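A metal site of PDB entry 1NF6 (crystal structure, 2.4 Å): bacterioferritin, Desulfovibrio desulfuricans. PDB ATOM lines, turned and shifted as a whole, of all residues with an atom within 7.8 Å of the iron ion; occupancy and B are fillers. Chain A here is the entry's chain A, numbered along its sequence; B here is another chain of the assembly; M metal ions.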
ATOM      1  N   GLU A  23       8.215   2.677 -34.009  1.00  0.00           N
ATOM      2  CA  GLU A  23       7.338   1.590 -33.569  1.00  0.00           C
ATOM      3  C   GLU A  23       8.160   0.346 -33.249  1.00  0.00           C
ATOM      4  O   GLU A  23       7.882  -0.383 -32.293  1.00  0.00           O
ATOM      5  CB  GLU A  23       6.264   1.282 -34.614  1.00  0.00           C
ATOM      6  CG  GLU A  23       5.285   2.409 -34.908  1.00  0.00           C
ATOM      7  CD  GLU A  23       4.323   2.645 -33.754  1.00  0.00           C
ATOM      8  OE1 GLU A  23       4.448   1.885 -32.760  1.00  0.00           O
ATOM      9  OE2 GLU A  23       3.465   3.552 -33.788  1.00  0.00           O
ATOM     10  N   ALA A  26       9.566   0.829 -29.656  1.00  0.00           N
ATOM     11  CA  ALA A  26       8.486   0.731 -28.702  1.00  0.00           C
ATOM     12  C   ALA A  26       8.036  -0.703 -28.487  1.00  0.00           C
ATOM     13  O   ALA A  26       7.678  -1.073 -27.370  1.00  0.00           O
ATOM     14  CB  ALA A  26       7.296   1.561 -29.185  1.00  0.00           C
ATOM     15  N   TYR A  30       8.615  -1.730 -24.798  1.00  0.00           N
ATOM     16  CA  TYR A  30       7.443  -2.164 -24.045  1.00  0.00           C
ATOM     17  C   TYR A  30       7.516  -3.643 -23.671  1.00  0.00           C
ATOM     18  O   TYR A  30       7.186  -4.023 -22.552  1.00  0.00           O
ATOM     19  CB  TYR A  30       6.164  -1.863 -24.839  1.00  0.00           C
ATOM     20  CG  TYR A  30       5.989  -0.384 -25.084  1.00  0.00           C
ATOM     21  CD1 TYR A  30       5.120   0.113 -26.035  1.00  0.00           C
ATOM     22  CD2 TYR A  30       6.720   0.530 -24.332  1.00  0.00           C
ATOM     23  CE1 TYR A  30       4.987   1.480 -26.229  1.00  0.00           C
ATOM     24  CE2 TYR A  30       6.601   1.900 -24.508  1.00  0.00           C
ATOM     25  CZ  TYR A  30       5.724   2.363 -25.469  1.00  0.00           C
ATOM     26  OH  TYR A  30       5.608   3.728 -25.658  1.00  0.00           O
ATOM     27  N   ILE A  52      -0.420  -3.196 -25.392  1.00  0.00           N
ATOM     28  CA  ILE A  52      -0.048  -1.966 -26.094  1.00  0.00           C
ATOM     29  C   ILE A  52       1.110  -2.227 -27.052  1.00  0.00           C
ATOM     30  O   ILE A  52       1.159  -1.659 -28.135  1.00  0.00           O
ATOM     31  CB  ILE A  52       0.283  -0.847 -25.086  1.00  0.00           C
ATOM     32  CG1 ILE A  52      -0.946  -0.374 -24.310  1.00  0.00           C
ATOM     33  CG2 ILE A  52       0.979   0.319 -25.768  1.00  0.00           C
ATOM     34  CD1 ILE A  52      -0.636   0.547 -23.155  1.00  0.00           C
ATOM     35  N   ALA A  53       2.026  -3.102 -26.672  1.00  0.00           N
ATOM     36  CA  ALA A  53       3.096  -3.495 -27.597  1.00  0.00           C
ATOM     37  C   ALA A  53       2.515  -4.092 -28.878  1.00  0.00           C
ATOM     38  O   ALA A  53       3.003  -3.838 -29.978  1.00  0.00           O
ATOM     39  CB  ALA A  53       4.041  -4.492 -26.926  1.00  0.00           C
ATOM     40  N   ASP A  55      -0.398  -3.403 -30.125  1.00  0.00           N
ATOM     41  CA  ASP A  55      -0.911  -2.260 -30.862  1.00  0.00           C
ATOM     42  C   ASP A  55       0.204  -1.599 -31.668  1.00  0.00           C
ATOM     43  O   ASP A  55      -0.024  -1.188 -32.812  1.00  0.00           O
ATOM     44  CB  ASP A  55      -1.543  -1.229 -29.939  1.00  0.00           C
ATOM     45  CG  ASP A  55      -2.875  -1.613 -29.321  1.00  0.00           C
ATOM     46  OD1 ASP A  55      -3.494  -2.613 -29.742  1.00  0.00           O
ATOM     47  OD2 ASP A  55      -3.313  -0.920 -28.369  1.00  0.00           O
ATOM     48  N   GLU A  56       1.397  -1.487 -31.102  1.00  0.00           N
ATOM     49  CA  GLU A  56       2.564  -0.910 -31.747  1.00  0.00           C
ATOM     50  C   GLU A  56       3.060  -1.774 -32.902  1.00  0.00           C
ATOM     51  O   GLU A  56       3.551  -1.274 -33.914  1.00  0.00           O
ATOM     52  CB  GLU A  56       3.721  -0.694 -30.761  1.00  0.00           C
ATOM     53  CG  GLU A  56       3.378  -0.031 -29.450  1.00  0.00           C
ATOM     54  CD  GLU A  56       2.640   1.279 -29.585  1.00  0.00           C
ATOM     55  OE1 GLU A  56       1.749   1.414 -30.441  1.00  0.00           O
ATOM     56  OE2 GLU A  56       2.943   2.210 -28.807  1.00  0.00           O
ATOM     57  N   HIS A  59       0.768  -1.058 -35.662  1.00  0.00           N
ATOM     58  CA  HIS A  59       1.258   0.199 -36.232  1.00  0.00           C
ATOM     59  C   HIS A  59       2.395  -0.049 -37.216  1.00  0.00           C
ATOM     60  O   HIS A  59       2.326   0.354 -38.369  1.00  0.00           O
ATOM     61  CB  HIS A  59       1.725   1.154 -35.121  1.00  0.00           C
ATOM     62  CG  HIS A  59       0.605   1.639 -34.255  1.00  0.00           C
ATOM     63  ND1 HIS A  59       0.811   2.522 -33.216  1.00  0.00           N
ATOM     64  CD2 HIS A  59      -0.721   1.361 -34.254  1.00  0.00           C
ATOM     65  CE1 HIS A  59      -0.350   2.783 -32.615  1.00  0.00           C
ATOM     66  NE2 HIS A  59      -1.283   2.085 -33.232  1.00  0.00           N
ATOM     67  N   ASP A  95       7.527   5.765 -20.503  1.00  0.00           N
ATOM     68  CA  ASP A  95       6.574   5.432 -21.557  1.00  0.00           C
ATOM     69  C   ASP A  95       5.632   6.596 -21.836  1.00  0.00           C
ATOM     70  O   ASP A  95       5.314   6.882 -22.999  1.00  0.00           O
ATOM     71  CB  ASP A  95       5.783   4.174 -21.188  1.00  0.00           C
ATOM     72  CG  ASP A  95       6.673   2.943 -21.167  1.00  0.00           C
ATOM     73  OD1 ASP A  95       7.851   3.081 -21.549  1.00  0.00           O
ATOM     74  OD2 ASP A  95       6.191   1.861 -20.777  1.00  0.00           O
ATOM     75  N   GLN A  98       7.555   8.843 -23.946  1.00  0.00           N
ATOM     76  CA  GLN A  98       7.705   8.313 -25.304  1.00  0.00           C
ATOM     77  C   GLN A  98       6.440   8.467 -26.131  1.00  0.00           C
ATOM     78  O   GLN A  98       6.497   8.901 -27.287  1.00  0.00           O
ATOM     79  CB  GLN A  98       8.106   6.840 -25.256  1.00  0.00           C
ATOM     80  CG  GLN A  98       8.413   6.223 -26.611  1.00  0.00           C
ATOM     81  CD  GLN A  98       9.080   4.863 -26.486  1.00  0.00           C
ATOM     82  OE1 GLN A  98       9.664   4.562 -25.456  1.00  0.00           O
ATOM     83  NE2 GLN A  98       9.016   4.047 -27.540  1.00  0.00           N
ATOM     84  N   GLU A  99       5.288   8.114 -25.560  1.00  0.00           N
ATOM     85  CA  GLU A  99       4.039   8.213 -26.320  1.00  0.00           C
ATOM     86  C   GLU A  99       3.788   9.657 -26.724  1.00  0.00           C
ATOM     87  O   GLU A  99       3.312   9.962 -27.812  1.00  0.00           O
ATOM     88  CB  GLU A  99       2.866   7.678 -25.505  1.00  0.00           C
ATOM     89  CG  GLU A  99       2.875   6.173 -25.261  1.00  0.00           C
ATOM     90  CD  GLU A  99       2.857   5.363 -26.544  1.00  0.00           C
ATOM     91  OE1 GLU A  99       1.896   5.480 -27.329  1.00  0.00           O
ATOM     92  OE2 GLU A  99       3.821   4.606 -26.792  1.00  0.00           O
ATOM     93  N   THR A 102       6.277  10.477 -29.396  1.00  0.00           N
ATOM     94  CA  THR A 102       5.834   9.846 -30.632  1.00  0.00           C
ATOM     95  C   THR A 102       4.738  10.664 -31.303  1.00  0.00           C
ATOM     96  O   THR A 102       4.834  10.962 -32.492  1.00  0.00           O
ATOM     97  CB  THR A 102       5.324   8.421 -30.395  1.00  0.00           C
ATOM     98  OG1 THR A 102       6.361   7.634 -29.798  1.00  0.00           O
ATOM     99  CG2 THR A 102       4.957   7.765 -31.714  1.00  0.00           C
ATOM    100  N   ILE A 103       3.725  11.020 -30.514  1.00  0.00           N
ATOM    101  CA  ILE A 103       2.610  11.838 -30.968  1.00  0.00           C
ATOM    102  C   ILE A 103       3.128  13.137 -31.598  1.00  0.00           C
ATOM    103  O   ILE A 103       2.725  13.488 -32.705  1.00  0.00           O
ATOM    104  CB  ILE A 103       1.647  12.161 -29.813  1.00  0.00           C
ATOM    105  CG1 ILE A 103       0.811  10.965 -29.339  1.00  0.00           C
ATOM    106  CG2 ILE A 103       0.711  13.315 -30.182  1.00  0.00           C
ATOM    107  CD1 ILE A 103      -0.018  11.248 -28.098  1.00  0.00           C
ATOM    108  N   TYR A 106       4.714  12.072 -34.931  1.00  0.00           N
ATOM    109  CA  TYR A 106       3.788  11.626 -35.968  1.00  0.00           C
ATOM    110  C   TYR A 106       3.050  12.815 -36.569  1.00  0.00           C
ATOM    111  O   TYR A 106       2.737  12.817 -37.762  1.00  0.00           O
ATOM    112  CB  TYR A 106       2.797  10.600 -35.414  1.00  0.00           C
ATOM    113  CG  TYR A 106       3.370   9.222 -35.199  1.00  0.00           C
ATOM    114  CD1 TYR A 106       4.726   8.984 -35.428  1.00  0.00           C
ATOM    115  CD2 TYR A 106       2.589   8.163 -34.766  1.00  0.00           C
ATOM    116  CE1 TYR A 106       5.259   7.727 -35.228  1.00  0.00           C
ATOM    117  CE2 TYR A 106       3.122   6.907 -34.566  1.00  0.00           C
ATOM    118  CZ  TYR A 106       4.463   6.685 -34.798  1.00  0.00           C
ATOM    119  OH  TYR A 106       5.017   5.434 -34.604  1.00  0.00           O
ATOM    120  N   ILE A 128      -3.484   6.487 -36.255  1.00  0.00           N
ATOM    121  CA  ILE A 128      -2.514   5.937 -35.305  1.00  0.00           C
ATOM    122  C   ILE A 128      -2.204   6.913 -34.183  1.00  0.00           C
ATOM    123  O   ILE A 128      -1.823   6.508 -33.087  1.00  0.00           O
ATOM    124  CB  ILE A 128      -1.242   5.507 -36.060  1.00  0.00           C
ATOM    125  CG1 ILE A 128      -1.426   4.196 -36.823  1.00  0.00           C
ATOM    126  CG2 ILE A 128      -0.037   5.431 -35.130  1.00  0.00           C
ATOM    127  CD1 ILE A 128      -0.278   3.852 -37.745  1.00  0.00           C
ATOM    128  N   ILE A 129      -2.356   8.203 -34.433  1.00  0.00           N
ATOM    129  CA  ILE A 129      -2.079   9.202 -33.399  1.00  0.00           C
ATOM    130  C   ILE A 129      -3.162   9.159 -32.319  1.00  0.00           C
ATOM    131  O   ILE A 129      -2.895   9.444 -31.148  1.00  0.00           O
ATOM    132  CB  ILE A 129      -1.972  10.615 -33.996  1.00  0.00           C
ATOM    133  CG1 ILE A 129      -0.661  10.897 -34.738  1.00  0.00           C
ATOM    134  CG2 ILE A 129      -2.200  11.663 -32.904  1.00  0.00           C
ATOM    135  CD1 ILE A 129      -0.717  12.115 -35.622  1.00  0.00           C
ATOM    136  N   GLU A 131      -4.808   6.406 -31.313  1.00  0.00           N
ATOM    137  CA  GLU A 131      -4.399   5.253 -30.531  1.00  0.00           C
ATOM    138  C   GLU A 131      -3.244   5.593 -29.609  1.00  0.00           C
ATOM    139  O   GLU A 131      -3.260   5.271 -28.416  1.00  0.00           O
ATOM    140  CB  GLU A 131      -4.022   4.096 -31.454  1.00  0.00           C
ATOM    141  CG  GLU A 131      -5.098   3.740 -32.470  1.00  0.00           C
ATOM    142  CD  GLU A 131      -4.827   2.436 -33.191  1.00  0.00           C
ATOM    143  OE1 GLU A 131      -3.729   1.882 -32.979  1.00  0.00           O
ATOM    144  OE2 GLU A 131      -5.695   1.974 -33.948  1.00  0.00           O
ATOM    145  N   GLU A 132      -2.222   6.262 -30.146  1.00  0.00           N
ATOM    146  CA  GLU A 132      -1.112   6.704 -29.312  1.00  0.00           C
ATOM    147  C   GLU A 132      -1.612   7.544 -28.131  1.00  0.00           C
ATOM    148  O   GLU A 132      -1.094   7.467 -27.019  1.00  0.00           O
ATOM    149  CB  GLU A 132      -0.111   7.495 -30.145  1.00  0.00           C
ATOM    150  CG  GLU A 132       0.578   6.665 -31.218  1.00  0.00           C
ATOM    151  CD  GLU A 132       1.459   5.556 -30.677  1.00  0.00           C
ATOM    152  OE1 GLU A 132       0.924   4.553 -30.144  1.00  0.00           O
ATOM    153  OE2 GLU A 132       2.698   5.656 -30.775  1.00  0.00           O
ATOM    154  N   GLN A 133      -2.650   8.340 -28.376  1.00  0.00           N
ATOM    155  CA  GLN A 133      -3.250   9.147 -27.305  1.00  0.00           C
ATOM    156  C   GLN A 133      -3.918   8.232 -26.279  1.00  0.00           C
ATOM    157  O   GLN A 133      -3.866   8.511 -25.074  1.00  0.00           O
ATOM    158  CB  GLN A 133      -4.246  10.150 -27.879  1.00  0.00           C
ATOM    159  CG  GLN A 133      -5.000  10.988 -26.871  1.00  0.00           C
ATOM    160  CD  GLN A 133      -4.124  11.923 -26.065  1.00  0.00           C
ATOM    161  OE1 GLN A 133      -3.615  12.932 -26.566  1.00  0.00           O
ATOM    162  NE2 GLN A 133      -3.924  11.606 -24.795  1.00  0.00           N
ATOM    163  N   ALA A 134      -4.514   7.135 -26.738  1.00  0.00           N
ATOM    164  CA  ALA A 134      -5.117   6.183 -25.809  1.00  0.00           C
ATOM    165  C   ALA A 134      -4.047   5.554 -24.928  1.00  0.00           C
ATOM    166  O   ALA A 134      -4.249   5.316 -23.743  1.00  0.00           O
ATOM    167  CB  ALA A 134      -5.902   5.115 -26.552  1.00  0.00           C
ATOM    168  N   HIS A 135      -2.904   5.282 -25.537  1.00  0.00           N
ATOM    169  CA  HIS A 135      -1.745   4.735 -24.848  1.00  0.00           C
ATOM    170  C   HIS A 135      -1.135   5.738 -23.877  1.00  0.00           C
ATOM    171  O   HIS A 135      -0.772   5.389 -22.755  1.00  0.00           O
ATOM    172  CB  HIS A 135      -0.688   4.306 -25.871  1.00  0.00           C
ATOM    173  CG  HIS A 135      -1.104   3.181 -26.776  1.00  0.00           C
ATOM    174  ND1 HIS A 135      -0.406   2.861 -27.910  1.00  0.00           N
ATOM    175  CD2 HIS A 135      -2.130   2.313 -26.711  1.00  0.00           C
ATOM    176  CE1 HIS A 135      -0.973   1.838 -28.506  1.00  0.00           C
ATOM    177  NE2 HIS A 135      -2.027   1.473 -27.813  1.00  0.00           N
ATOM    178  N   LEU A 136      -0.997   6.994 -24.294  1.00  0.00           N
ATOM    179  CA  LEU A 136      -0.460   8.041 -23.430  1.00  0.00           C
ATOM    180  C   LEU A 136      -1.351   8.239 -22.204  1.00  0.00           C
ATOM    181  O   LEU A 136      -0.855   8.365 -21.085  1.00  0.00           O
ATOM    182  CB  LEU A 136      -0.312   9.353 -24.202  1.00  0.00           C
ATOM    183  CG  LEU A 136      -0.022  10.620 -23.404  1.00  0.00           C
ATOM    184  CD1 LEU A 136       1.270  10.475 -22.606  1.00  0.00           C
ATOM    185  CD2 LEU A 136       0.050  11.830 -24.320  1.00  0.00           C
ATOM    186  N   TYR A 139      -0.681   5.325 -19.615  1.00  0.00           N
ATOM    187  CA  TYR A 139       0.575   5.348 -18.861  1.00  0.00           C
ATOM    188  C   TYR A 139       0.621   6.477 -17.825  1.00  0.00           C
ATOM    189  O   TYR A 139       1.206   6.307 -16.759  1.00  0.00           O
ATOM    190  CB  TYR A 139       1.743   5.489 -19.832  1.00  0.00           C
ATOM    191  CG  TYR A 139       2.064   4.284 -20.682  1.00  0.00           C
ATOM    192  CD1 TYR A 139       2.355   4.400 -22.030  1.00  0.00           C
ATOM    193  CD2 TYR A 139       2.073   3.009 -20.130  1.00  0.00           C
ATOM    194  CE1 TYR A 139       2.652   3.295 -22.812  1.00  0.00           C
ATOM    195  CE2 TYR A 139       2.363   1.902 -20.888  1.00  0.00           C
ATOM    196  CZ  TYR A 139       2.656   2.045 -22.233  1.00  0.00           C
ATOM    197  OH  TYR A 139       2.946   0.922 -22.976  1.00  0.00           O
ATOM    198  N   VAL B 172      -6.114  -0.833 -27.676  1.00  0.00           N
ATOM    199  CA  VAL B 172      -7.242   0.042 -28.016  1.00  0.00           C
ATOM    200  C   VAL B 172      -8.447  -0.760 -28.511  1.00  0.00           C
ATOM    201  O   VAL B 172      -8.322  -1.983 -28.629  1.00  0.00           O
ATOM    202  CB  VAL B 172      -6.866   1.054 -29.117  1.00  0.00           C
ATOM    203  CG1 VAL B 172      -5.800   2.008 -28.633  1.00  0.00           C
ATOM    204  CG2 VAL B 172      -6.424   0.309 -30.369  1.00  0.00           C
HETATM  205 FE    FE M   1       1.483   3.645 -28.546  1.00  0.00          FE
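A ring nitrogen (NE2) of His 135 lies within hydrogen-bond range of the side-chain carboxylate (OD2) of Asp 55 (2.8 Å).
A ring nitrogen (ND1) of His 59 is in hydrogen-bond range of the side-chain carboxylate of Glu 56 (3.1 Å).
Four residues have an atom within 4 Å of the iron ion: Glu 56, Glu 99, Glu 132 and His 135.
The nearest printed residue that does not touch the iron ion is Ile 52 (4.4 Å).
The iron ion is bound by the side-chain carboxylate (OE1) of Glu 132, the side-chain carboxylate (OE2) of Glu 56, a ring nitrogen (ND1) of His 135 and the side-chain carboxylate (OE1) of Glu 99.
The iron ion has four donor atoms within binding distance.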
